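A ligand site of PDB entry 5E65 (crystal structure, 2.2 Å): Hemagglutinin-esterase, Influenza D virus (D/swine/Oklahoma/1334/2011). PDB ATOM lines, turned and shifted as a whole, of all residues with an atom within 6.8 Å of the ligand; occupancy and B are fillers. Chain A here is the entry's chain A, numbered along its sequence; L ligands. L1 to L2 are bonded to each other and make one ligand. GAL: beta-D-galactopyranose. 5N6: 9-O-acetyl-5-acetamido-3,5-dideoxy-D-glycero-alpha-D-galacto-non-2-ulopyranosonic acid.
CZ of Phe 125 touches O8 of 5N6 L2, 3.5 Å away. CA of Gly 168 touches C11 of 5N6 L2, 3.6 Å away. Ala 170 touches the ligand. Trp 183 touches the ligand. Ala 185 touches the ligand. Phe 238 touches the ligand. Val 273 touches the ligand. CE2 of Phe 295 touches OBJ of 5N6 L2, at 3.0 Å. Within 4 Å of the ligand: Phe 125, Gly 168, Thr 169, Ala 170, Ser 171, Trp 183, Ala 185, Tyr 229, Phe 238, Val 273 and Phe 295. The nearest printed residue that does not touch the ligand is Phe 227 (4.2 Å).
The side-chain hydroxyl (OH) of Tyr 229 lies within hydrogen-bond range of an oxygen (OBJ) of 5N6 L2. An oxygen (O1A) of 5N6 L2 is in hydrogen-bond range of the side-chain hydroxyl of Ser 171, 3.4 Å away. N5 of 5N6 L2 sits at hydrogen-bond distance from O of Thr 169. N of Ser 171 is in hydrogen-bond range of O1A of 5N6 L2 (2.8 Å).
The backbone carbonyl oxygen (O) of Thr 166 is in hydrogen-bond range of the backbone NH (N) of Ala 185 (2.8 Å). N of Gly 168 is in hydrogen-bond range of O of Trp 183, 2.6 Å away. O of Ala 170 is in hydrogen-bond range of N of Ser 175 (3.0 Å).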
ATOM      1  N   PHE A 125      18.167 -29.432 -12.852  1.00  0.00           N
ATOM      2  CA  PHE A 125      16.937 -30.203 -13.106  1.00  0.00           C
ATOM      3  C   PHE A 125      16.786 -30.648 -14.567  1.00  0.00           C
ATOM      4  O   PHE A 125      15.702 -31.029 -14.985  1.00  0.00           O
ATOM      5  CB  PHE A 125      15.691 -29.399 -12.703  1.00  0.00           C
ATOM      6  CG  PHE A 125      15.668 -29.001 -11.259  1.00  0.00           C
ATOM      7  CD1 PHE A 125      16.091 -29.865 -10.276  1.00  0.00           C
ATOM      8  CD2 PHE A 125      15.205 -27.742 -10.896  1.00  0.00           C
ATOM      9  CE1 PHE A 125      16.060 -29.487  -8.938  1.00  0.00           C
ATOM     10  CE2 PHE A 125      15.179 -27.357  -9.568  1.00  0.00           C
ATOM     11  CZ  PHE A 125      15.606 -28.229  -8.589  1.00  0.00           C
ATOM     12  N   THR A 166       9.180 -14.655  -5.956  1.00  0.00           N
ATOM     13  CA  THR A 166      10.582 -14.289  -5.872  1.00  0.00           C
ATOM     14  C   THR A 166      11.461 -15.177  -6.750  1.00  0.00           C
ATOM     15  O   THR A 166      11.021 -16.228  -7.220  1.00  0.00           O
ATOM     16  CB  THR A 166      11.091 -14.362  -4.420  1.00  0.00           C
ATOM     17  OG1 THR A 166      10.786 -15.645  -3.871  1.00  0.00           O
ATOM     18  CG2 THR A 166      10.436 -13.283  -3.571  1.00  0.00           C
ATOM     19  N   ALA A 167      12.705 -14.756  -6.969  1.00  0.00           N
ATOM     20  CA  ALA A 167      13.616 -15.441  -7.877  1.00  0.00           C
ATOM     21  C   ALA A 167      13.994 -16.844  -7.388  1.00  0.00           C
ATOM     22  O   ALA A 167      14.245 -17.046  -6.211  1.00  0.00           O
ATOM     23  CB  ALA A 167      14.873 -14.604  -8.086  1.00  0.00           C
ATOM     24  N   GLY A 168      14.039 -17.793  -8.315  1.00  0.00           N
ATOM     25  CA  GLY A 168      14.278 -19.187  -7.983  1.00  0.00           C
ATOM     26  C   GLY A 168      15.737 -19.615  -7.857  1.00  0.00           C
ATOM     27  O   GLY A 168      16.598 -19.133  -8.584  1.00  0.00           O
ATOM     28  N   THR A 169      15.983 -20.532  -6.926  1.00  0.00           N
ATOM     29  CA  THR A 169      17.333 -21.027  -6.656  1.00  0.00           C
ATOM     30  C   THR A 169      17.285 -22.540  -6.415  1.00  0.00           C
ATOM     31  O   THR A 169      16.343 -23.042  -5.811  1.00  0.00           O
ATOM     32  CB  THR A 169      17.946 -20.308  -5.446  1.00  0.00           C
ATOM     33  OG1 THR A 169      18.485 -19.048  -5.868  1.00  0.00           O
ATOM     34  CG2 THR A 169      19.061 -21.129  -4.795  1.00  0.00           C
ATOM     35  N   ALA A 170      18.292 -23.258  -6.908  1.00  0.00           N
ATOM     36  CA  ALA A 170      18.325 -24.710  -6.733  1.00  0.00           C
ATOM     37  C   ALA A 170      19.709 -25.252  -6.415  1.00  0.00           C
ATOM     38  O   ALA A 170      20.698 -24.863  -7.044  1.00  0.00           O
ATOM     39  CB  ALA A 170      17.777 -25.392  -7.978  1.00  0.00           C
ATOM     40  N   SER A 171      19.766 -26.173  -5.456  1.00  0.00           N
ATOM     41  CA  SER A 171      21.012 -26.844  -5.085  1.00  0.00           C
ATOM     42  C   SER A 171      21.652 -27.557  -6.283  1.00  0.00           C
ATOM     43  O   SER A 171      22.867 -27.692  -6.340  1.00  0.00           O
ATOM     44  CB  SER A 171      20.750 -27.871  -3.973  1.00  0.00           C
ATOM     45  OG  SER A 171      19.813 -28.852  -4.406  1.00  0.00           O
ATOM     46  N   SER A 172      20.835 -27.974  -7.249  1.00  0.00           N
ATOM     47  CA  SER A 172      21.311 -28.677  -8.424  1.00  0.00           C
ATOM     48  C   SER A 172      21.872 -27.723  -9.464  1.00  0.00           C
ATOM     49  O   SER A 172      22.488 -28.157 -10.450  1.00  0.00           O
ATOM     50  CB  SER A 172      20.196 -29.518  -9.019  1.00  0.00           C
ATOM     51  OG  SER A 172      19.109 -28.712  -9.437  1.00  0.00           O
ATOM     52  N   SER A 175      23.383 -23.594  -6.520  1.00  0.00           N
ATOM     53  CA  SER A 175      22.651 -22.742  -5.587  1.00  0.00           C
ATOM     54  C   SER A 175      22.275 -21.415  -6.229  1.00  0.00           C
ATOM     55  O   SER A 175      22.287 -20.373  -5.585  1.00  0.00           O
ATOM     56  CB  SER A 175      23.472 -22.517  -4.308  1.00  0.00           C
ATOM     57  OG  SER A 175      23.870 -23.740  -3.727  1.00  0.00           O
ATOM     58  N   TRP A 177      20.620 -20.054 -10.517  1.00  0.00           N
ATOM     59  CA  TRP A 177      19.755 -20.432 -11.619  1.00  0.00           C
ATOM     60  C   TRP A 177      20.264 -19.907 -12.975  1.00  0.00           C
ATOM     61  O   TRP A 177      21.146 -19.054 -13.032  1.00  0.00           O
ATOM     62  CB  TRP A 177      18.325 -19.951 -11.364  1.00  0.00           C
ATOM     63  CG  TRP A 177      17.350 -20.559 -12.315  1.00  0.00           C
ATOM     64  CD1 TRP A 177      16.572 -19.909 -13.226  1.00  0.00           C
ATOM     65  CD2 TRP A 177      17.068 -21.953 -12.471  1.00  0.00           C
ATOM     66  NE1 TRP A 177      15.819 -20.813 -13.939  1.00  0.00           N
ATOM     67  CE2 TRP A 177      16.110 -22.075 -13.490  1.00  0.00           C
ATOM     68  CE3 TRP A 177      17.542 -23.107 -11.839  1.00  0.00           C
ATOM     69  CZ2 TRP A 177      15.605 -23.317 -13.890  1.00  0.00           C
ATOM     70  CZ3 TRP A 177      17.042 -24.336 -12.236  1.00  0.00           C
ATOM     71  CH2 TRP A 177      16.078 -24.425 -13.252  1.00  0.00           C
ATOM     72  N   TRP A 183      13.232 -17.946 -13.163  1.00  0.00           N
ATOM     73  CA  TRP A 183      12.456 -18.826 -12.308  1.00  0.00           C
ATOM     74  C   TRP A 183      11.801 -18.029 -11.187  1.00  0.00           C
ATOM     75  O   TRP A 183      12.495 -17.424 -10.378  1.00  0.00           O
ATOM     76  CB  TRP A 183      13.347 -19.916 -11.735  1.00  0.00           C
ATOM     77  CG  TRP A 183      12.629 -21.000 -10.998  1.00  0.00           C
ATOM     78  CD1 TRP A 183      11.288 -21.228 -10.967  1.00  0.00           C
ATOM     79  CD2 TRP A 183      13.230 -22.005 -10.169  1.00  0.00           C
ATOM     80  NE1 TRP A 183      11.012 -22.320 -10.179  1.00  0.00           N
ATOM     81  CE2 TRP A 183      12.186 -22.815  -9.671  1.00  0.00           C
ATOM     82  CE3 TRP A 183      14.547 -22.307  -9.806  1.00  0.00           C
ATOM     83  CZ2 TRP A 183      12.417 -23.905  -8.842  1.00  0.00           C
ATOM     84  CZ3 TRP A 183      14.780 -23.376  -8.970  1.00  0.00           C
ATOM     85  CH2 TRP A 183      13.721 -24.169  -8.493  1.00  0.00           C
ATOM     86  N   TYR A 184      10.476 -18.017 -11.154  1.00  0.00           N
ATOM     87  CA  TYR A 184       9.758 -17.297 -10.104  1.00  0.00           C
ATOM     88  C   TYR A 184       8.897 -18.240  -9.272  1.00  0.00           C
ATOM     89  O   TYR A 184       8.106 -19.016  -9.800  1.00  0.00           O
ATOM     90  CB  TYR A 184       8.889 -16.199 -10.717  1.00  0.00           C
ATOM     91  CG  TYR A 184       9.694 -15.042 -11.268  1.00  0.00           C
ATOM     92  CD1 TYR A 184      10.161 -14.041 -10.431  1.00  0.00           C
ATOM     93  CD2 TYR A 184       9.979 -14.965 -12.619  1.00  0.00           C
ATOM     94  CE1 TYR A 184      10.899 -12.977 -10.933  1.00  0.00           C
ATOM     95  CE2 TYR A 184      10.710 -13.910 -13.134  1.00  0.00           C
ATOM     96  CZ  TYR A 184      11.171 -12.918 -12.286  1.00  0.00           C
ATOM     97  OH  TYR A 184      11.901 -11.863 -12.800  1.00  0.00           O
ATOM     98  N   ALA A 185       9.059 -18.153  -7.956  1.00  0.00           N
ATOM     99  CA  ALA A 185       8.381 -19.066  -7.048  1.00  0.00           C
ATOM    100  C   ALA A 185       7.576 -18.331  -5.983  1.00  0.00           C
ATOM    101  O   ALA A 185       7.984 -17.293  -5.471  1.00  0.00           O
ATOM    102  CB  ALA A 185       9.394 -19.994  -6.397  1.00  0.00           C
ATOM    103  N   PHE A 227       8.191 -27.549 -16.351  1.00  0.00           N
ATOM    104  CA  PHE A 227       8.669 -28.583 -15.462  1.00  0.00           C
ATOM    105  C   PHE A 227       7.967 -29.909 -15.736  1.00  0.00           C
ATOM    106  O   PHE A 227       6.790 -29.938 -16.093  1.00  0.00           O
ATOM    107  CB  PHE A 227       8.478 -28.171 -14.004  1.00  0.00           C
ATOM    108  CG  PHE A 227       9.444 -27.117 -13.568  1.00  0.00           C
ATOM    109  CD1 PHE A 227      10.804 -27.375 -13.523  1.00  0.00           C
ATOM    110  CD2 PHE A 227       8.997 -25.860 -13.189  1.00  0.00           C
ATOM    111  CE1 PHE A 227      11.696 -26.403 -13.111  1.00  0.00           C
ATOM    112  CE2 PHE A 227       9.876 -24.886 -12.771  1.00  0.00           C
ATOM    113  CZ  PHE A 227      11.232 -25.161 -12.741  1.00  0.00           C
ATOM    114  N   TYR A 229       6.926 -33.536 -14.152  1.00  0.00           N
ATOM    115  CA  TYR A 229       6.702 -34.409 -12.999  1.00  0.00           C
ATOM    116  C   TYR A 229       6.232 -35.760 -13.531  1.00  0.00           C
ATOM    117  O   TYR A 229       5.757 -35.847 -14.657  1.00  0.00           O
ATOM    118  CB  TYR A 229       5.678 -33.804 -12.064  1.00  0.00           C
ATOM    119  CG  TYR A 229       6.072 -32.434 -11.564  1.00  0.00           C
ATOM    120  CD1 TYR A 229       6.678 -32.273 -10.326  1.00  0.00           C
ATOM    121  CD2 TYR A 229       5.862 -31.306 -12.354  1.00  0.00           C
ATOM    122  CE1 TYR A 229       7.059 -31.024  -9.886  1.00  0.00           C
ATOM    123  CE2 TYR A 229       6.243 -30.057 -11.914  1.00  0.00           C
ATOM    124  CZ  TYR A 229       6.830 -29.927 -10.680  1.00  0.00           C
ATOM    125  OH  TYR A 229       7.218 -28.684 -10.223  1.00  0.00           O
ATOM    126  N   PHE A 235       3.313 -34.336  -8.165  1.00  0.00           N
ATOM    127  CA  PHE A 235       3.266 -32.871  -8.308  1.00  0.00           C
ATOM    128  C   PHE A 235       2.586 -32.216  -7.127  1.00  0.00           C
ATOM    129  O   PHE A 235       2.976 -31.130  -6.693  1.00  0.00           O
ATOM    130  CB  PHE A 235       2.548 -32.449  -9.586  1.00  0.00           C
ATOM    131  CG  PHE A 235       2.400 -30.958  -9.702  1.00  0.00           C
ATOM    132  CD1 PHE A 235       3.491 -30.173 -10.024  1.00  0.00           C
ATOM    133  CD2 PHE A 235       1.174 -30.337  -9.487  1.00  0.00           C
ATOM    134  CE1 PHE A 235       3.378 -28.801 -10.118  1.00  0.00           C
ATOM    135  CE2 PHE A 235       1.058 -28.962  -9.590  1.00  0.00           C
ATOM    136  CZ  PHE A 235       2.160 -28.196  -9.912  1.00  0.00           C
ATOM    137  N   PHE A 238       4.003 -30.277  -4.293  1.00  0.00           N
ATOM    138  CA  PHE A 238       4.346 -28.855  -4.410  1.00  0.00           C
ATOM    139  C   PHE A 238       3.154 -27.949  -4.717  1.00  0.00           C
ATOM    140  O   PHE A 238       3.018 -26.886  -4.121  1.00  0.00           O
ATOM    141  CB  PHE A 238       5.416 -28.655  -5.480  1.00  0.00           C
ATOM    142  CG  PHE A 238       6.761 -29.214  -5.118  1.00  0.00           C
ATOM    143  CD1 PHE A 238       7.573 -28.554  -4.198  1.00  0.00           C
ATOM    144  CD2 PHE A 238       7.228 -30.383  -5.689  1.00  0.00           C
ATOM    145  CE1 PHE A 238       8.815 -29.062  -3.858  1.00  0.00           C
ATOM    146  CE2 PHE A 238       8.470 -30.896  -5.361  1.00  0.00           C
ATOM    147  CZ  PHE A 238       9.267 -30.229  -4.445  1.00  0.00           C
ATOM    148  N   VAL A 273      11.758 -34.071 -10.032  1.00  0.00           N
ATOM    149  CA  VAL A 273      11.395 -32.973 -10.920  1.00  0.00           C
ATOM    150  C   VAL A 273      12.450 -32.772 -12.006  1.00  0.00           C
ATOM    151  O   VAL A 273      13.653 -32.780 -11.741  1.00  0.00           O
ATOM    152  CB  VAL A 273      11.195 -31.650 -10.137  1.00  0.00           C
ATOM    153  CG1 VAL A 273      12.453 -31.272  -9.358  1.00  0.00           C
ATOM    154  CG2 VAL A 273      10.774 -30.527 -11.073  1.00  0.00           C
ATOM    155  N   ARG A 294       2.640 -21.928  -7.695  1.00  0.00           N
ATOM    156  CA  ARG A 294       3.940 -21.917  -7.042  1.00  0.00           C
ATOM    157  C   ARG A 294       5.123 -21.675  -8.004  1.00  0.00           C
ATOM    158  O   ARG A 294       6.057 -20.962  -7.645  1.00  0.00           O
ATOM    159  CB  ARG A 294       4.179 -23.228  -6.274  1.00  0.00           C
ATOM    160  CG  ARG A 294       5.588 -23.320  -5.723  1.00  0.00           C
ATOM    161  CD  ARG A 294       5.712 -24.219  -4.522  1.00  0.00           C
ATOM    162  NE  ARG A 294       6.919 -23.881  -3.760  1.00  0.00           N
ATOM    163  CZ  ARG A 294       7.300 -24.502  -2.649  1.00  0.00           C
ATOM    164  NH1 ARG A 294       6.588 -25.495  -2.165  1.00  0.00           N
ATOM    165  NH2 ARG A 294       8.410 -24.121  -2.026  1.00  0.00           N
ATOM    166  N   PHE A 295       5.069 -22.245  -9.197  1.00  0.00           N
ATOM    167  CA  PHE A 295       6.207 -22.136 -10.110  1.00  0.00           C
ATOM    168  C   PHE A 295       5.861 -21.459 -11.429  1.00  0.00           C
ATOM    169  O   PHE A 295       4.858 -21.786 -12.063  1.00  0.00           O
ATOM    170  CB  PHE A 295       6.808 -23.522 -10.370  1.00  0.00           C
ATOM    171  CG  PHE A 295       7.409 -24.148  -9.154  1.00  0.00           C
ATOM    172  CD1 PHE A 295       8.175 -23.400  -8.276  1.00  0.00           C
ATOM    173  CD2 PHE A 295       7.215 -25.492  -8.874  1.00  0.00           C
ATOM    174  CE1 PHE A 295       8.740 -23.970  -7.151  1.00  0.00           C
ATOM    175  CE2 PHE A 295       7.766 -26.080  -7.750  1.00  0.00           C
ATOM    176  CZ  PHE A 295       8.530 -25.312  -6.887  1.00  0.00           C
HETATM  177  C1  GAL L   1      14.366 -30.964  -1.724  1.00  0.00           C
HETATM  178  C2  GAL L   1      14.407 -29.495  -1.390  1.00  0.00           C
HETATM  179  C3  GAL L   1      15.475 -28.836  -2.156  1.00  0.00           C
HETATM  180  C4  GAL L   1      16.800 -29.524  -2.094  1.00  0.00           C
HETATM  181  C5  GAL L   1      16.687 -31.028  -2.175  1.00  0.00           C
HETATM  182  C6  GAL L   1      17.899 -31.661  -1.562  1.00  0.00           C
HETATM  183  O1  GAL L   1      13.394 -31.631  -0.908  1.00  0.00           O
HETATM  184  O2  GAL L   1      13.209 -28.854  -1.779  1.00  0.00           O
HETATM  185  O3  GAL L   1      15.648 -27.529  -1.660  1.00  0.00           O
HETATM  186  O4  GAL L   1      17.470 -29.061  -0.975  1.00  0.00           O
HETATM  187  O5  GAL L   1      15.641 -31.490  -1.392  1.00  0.00           O
HETATM  188  O6  GAL L   1      18.384 -32.671  -2.433  1.00  0.00           O
HETATM  189  CAF 5N6 L   2      11.514 -26.892  -8.959  1.00  0.00           C
HETATM  190  CAG 5N6 L   2      10.875 -27.875  -8.047  1.00  0.00           C
HETATM  191  C11 5N6 L   2      12.716 -21.721  -5.914  1.00  0.00           C
HETATM  192  C10 5N6 L   2      12.640 -22.921  -5.005  1.00  0.00           C
HETATM  193  C9  5N6 L   2      11.258 -27.582  -5.927  1.00  0.00           C
HETATM  194  C8  5N6 L   2      12.486 -27.432  -5.116  1.00  0.00           C
HETATM  195  C7  5N6 L   2      12.752 -25.960  -5.004  1.00  0.00           C
HETATM  196  N5  5N6 L   2      13.779 -23.267  -4.419  1.00  0.00           N
HETATM  197  C5  5N6 L   2      13.952 -24.364  -3.490  1.00  0.00           C
HETATM  198  C4  5N6 L   2      15.338 -24.187  -2.935  1.00  0.00           C
HETATM  199  C6  5N6 L   2      13.987 -25.658  -4.198  1.00  0.00           C
HETATM  200  C3  5N6 L   2      15.741 -25.257  -1.996  1.00  0.00           C
HETATM  201  C2  5N6 L   2      15.565 -26.551  -2.655  1.00  0.00           C
HETATM  202  C1  5N6 L   2      16.624 -26.743  -3.715  1.00  0.00           C
HETATM  203  OBJ 5N6 L   2       9.764 -28.287  -8.273  1.00  0.00           O
HETATM  204  O9  5N6 L   2      11.643 -28.270  -7.050  1.00  0.00           O
HETATM  205  O10 5N6 L   2      11.596 -23.527  -4.886  1.00  0.00           O
HETATM  206  O7  5N6 L   2      11.626 -25.360  -4.440  1.00  0.00           O
HETATM  207  O8  5N6 L   2      13.468 -28.010  -5.889  1.00  0.00           O
HETATM  208  O4  5N6 L   2      15.416 -23.005  -2.266  1.00  0.00           O
HETATM  209  O6  5N6 L   2      14.308 -26.666  -3.261  1.00  0.00           O
HETATM  210  O1B 5N6 L   2      16.294 -27.410  -4.688  1.00  0.00           O
HETATM  211  O1A 5N6 L   2      17.743 -26.285  -3.498  1.00  0.00           O
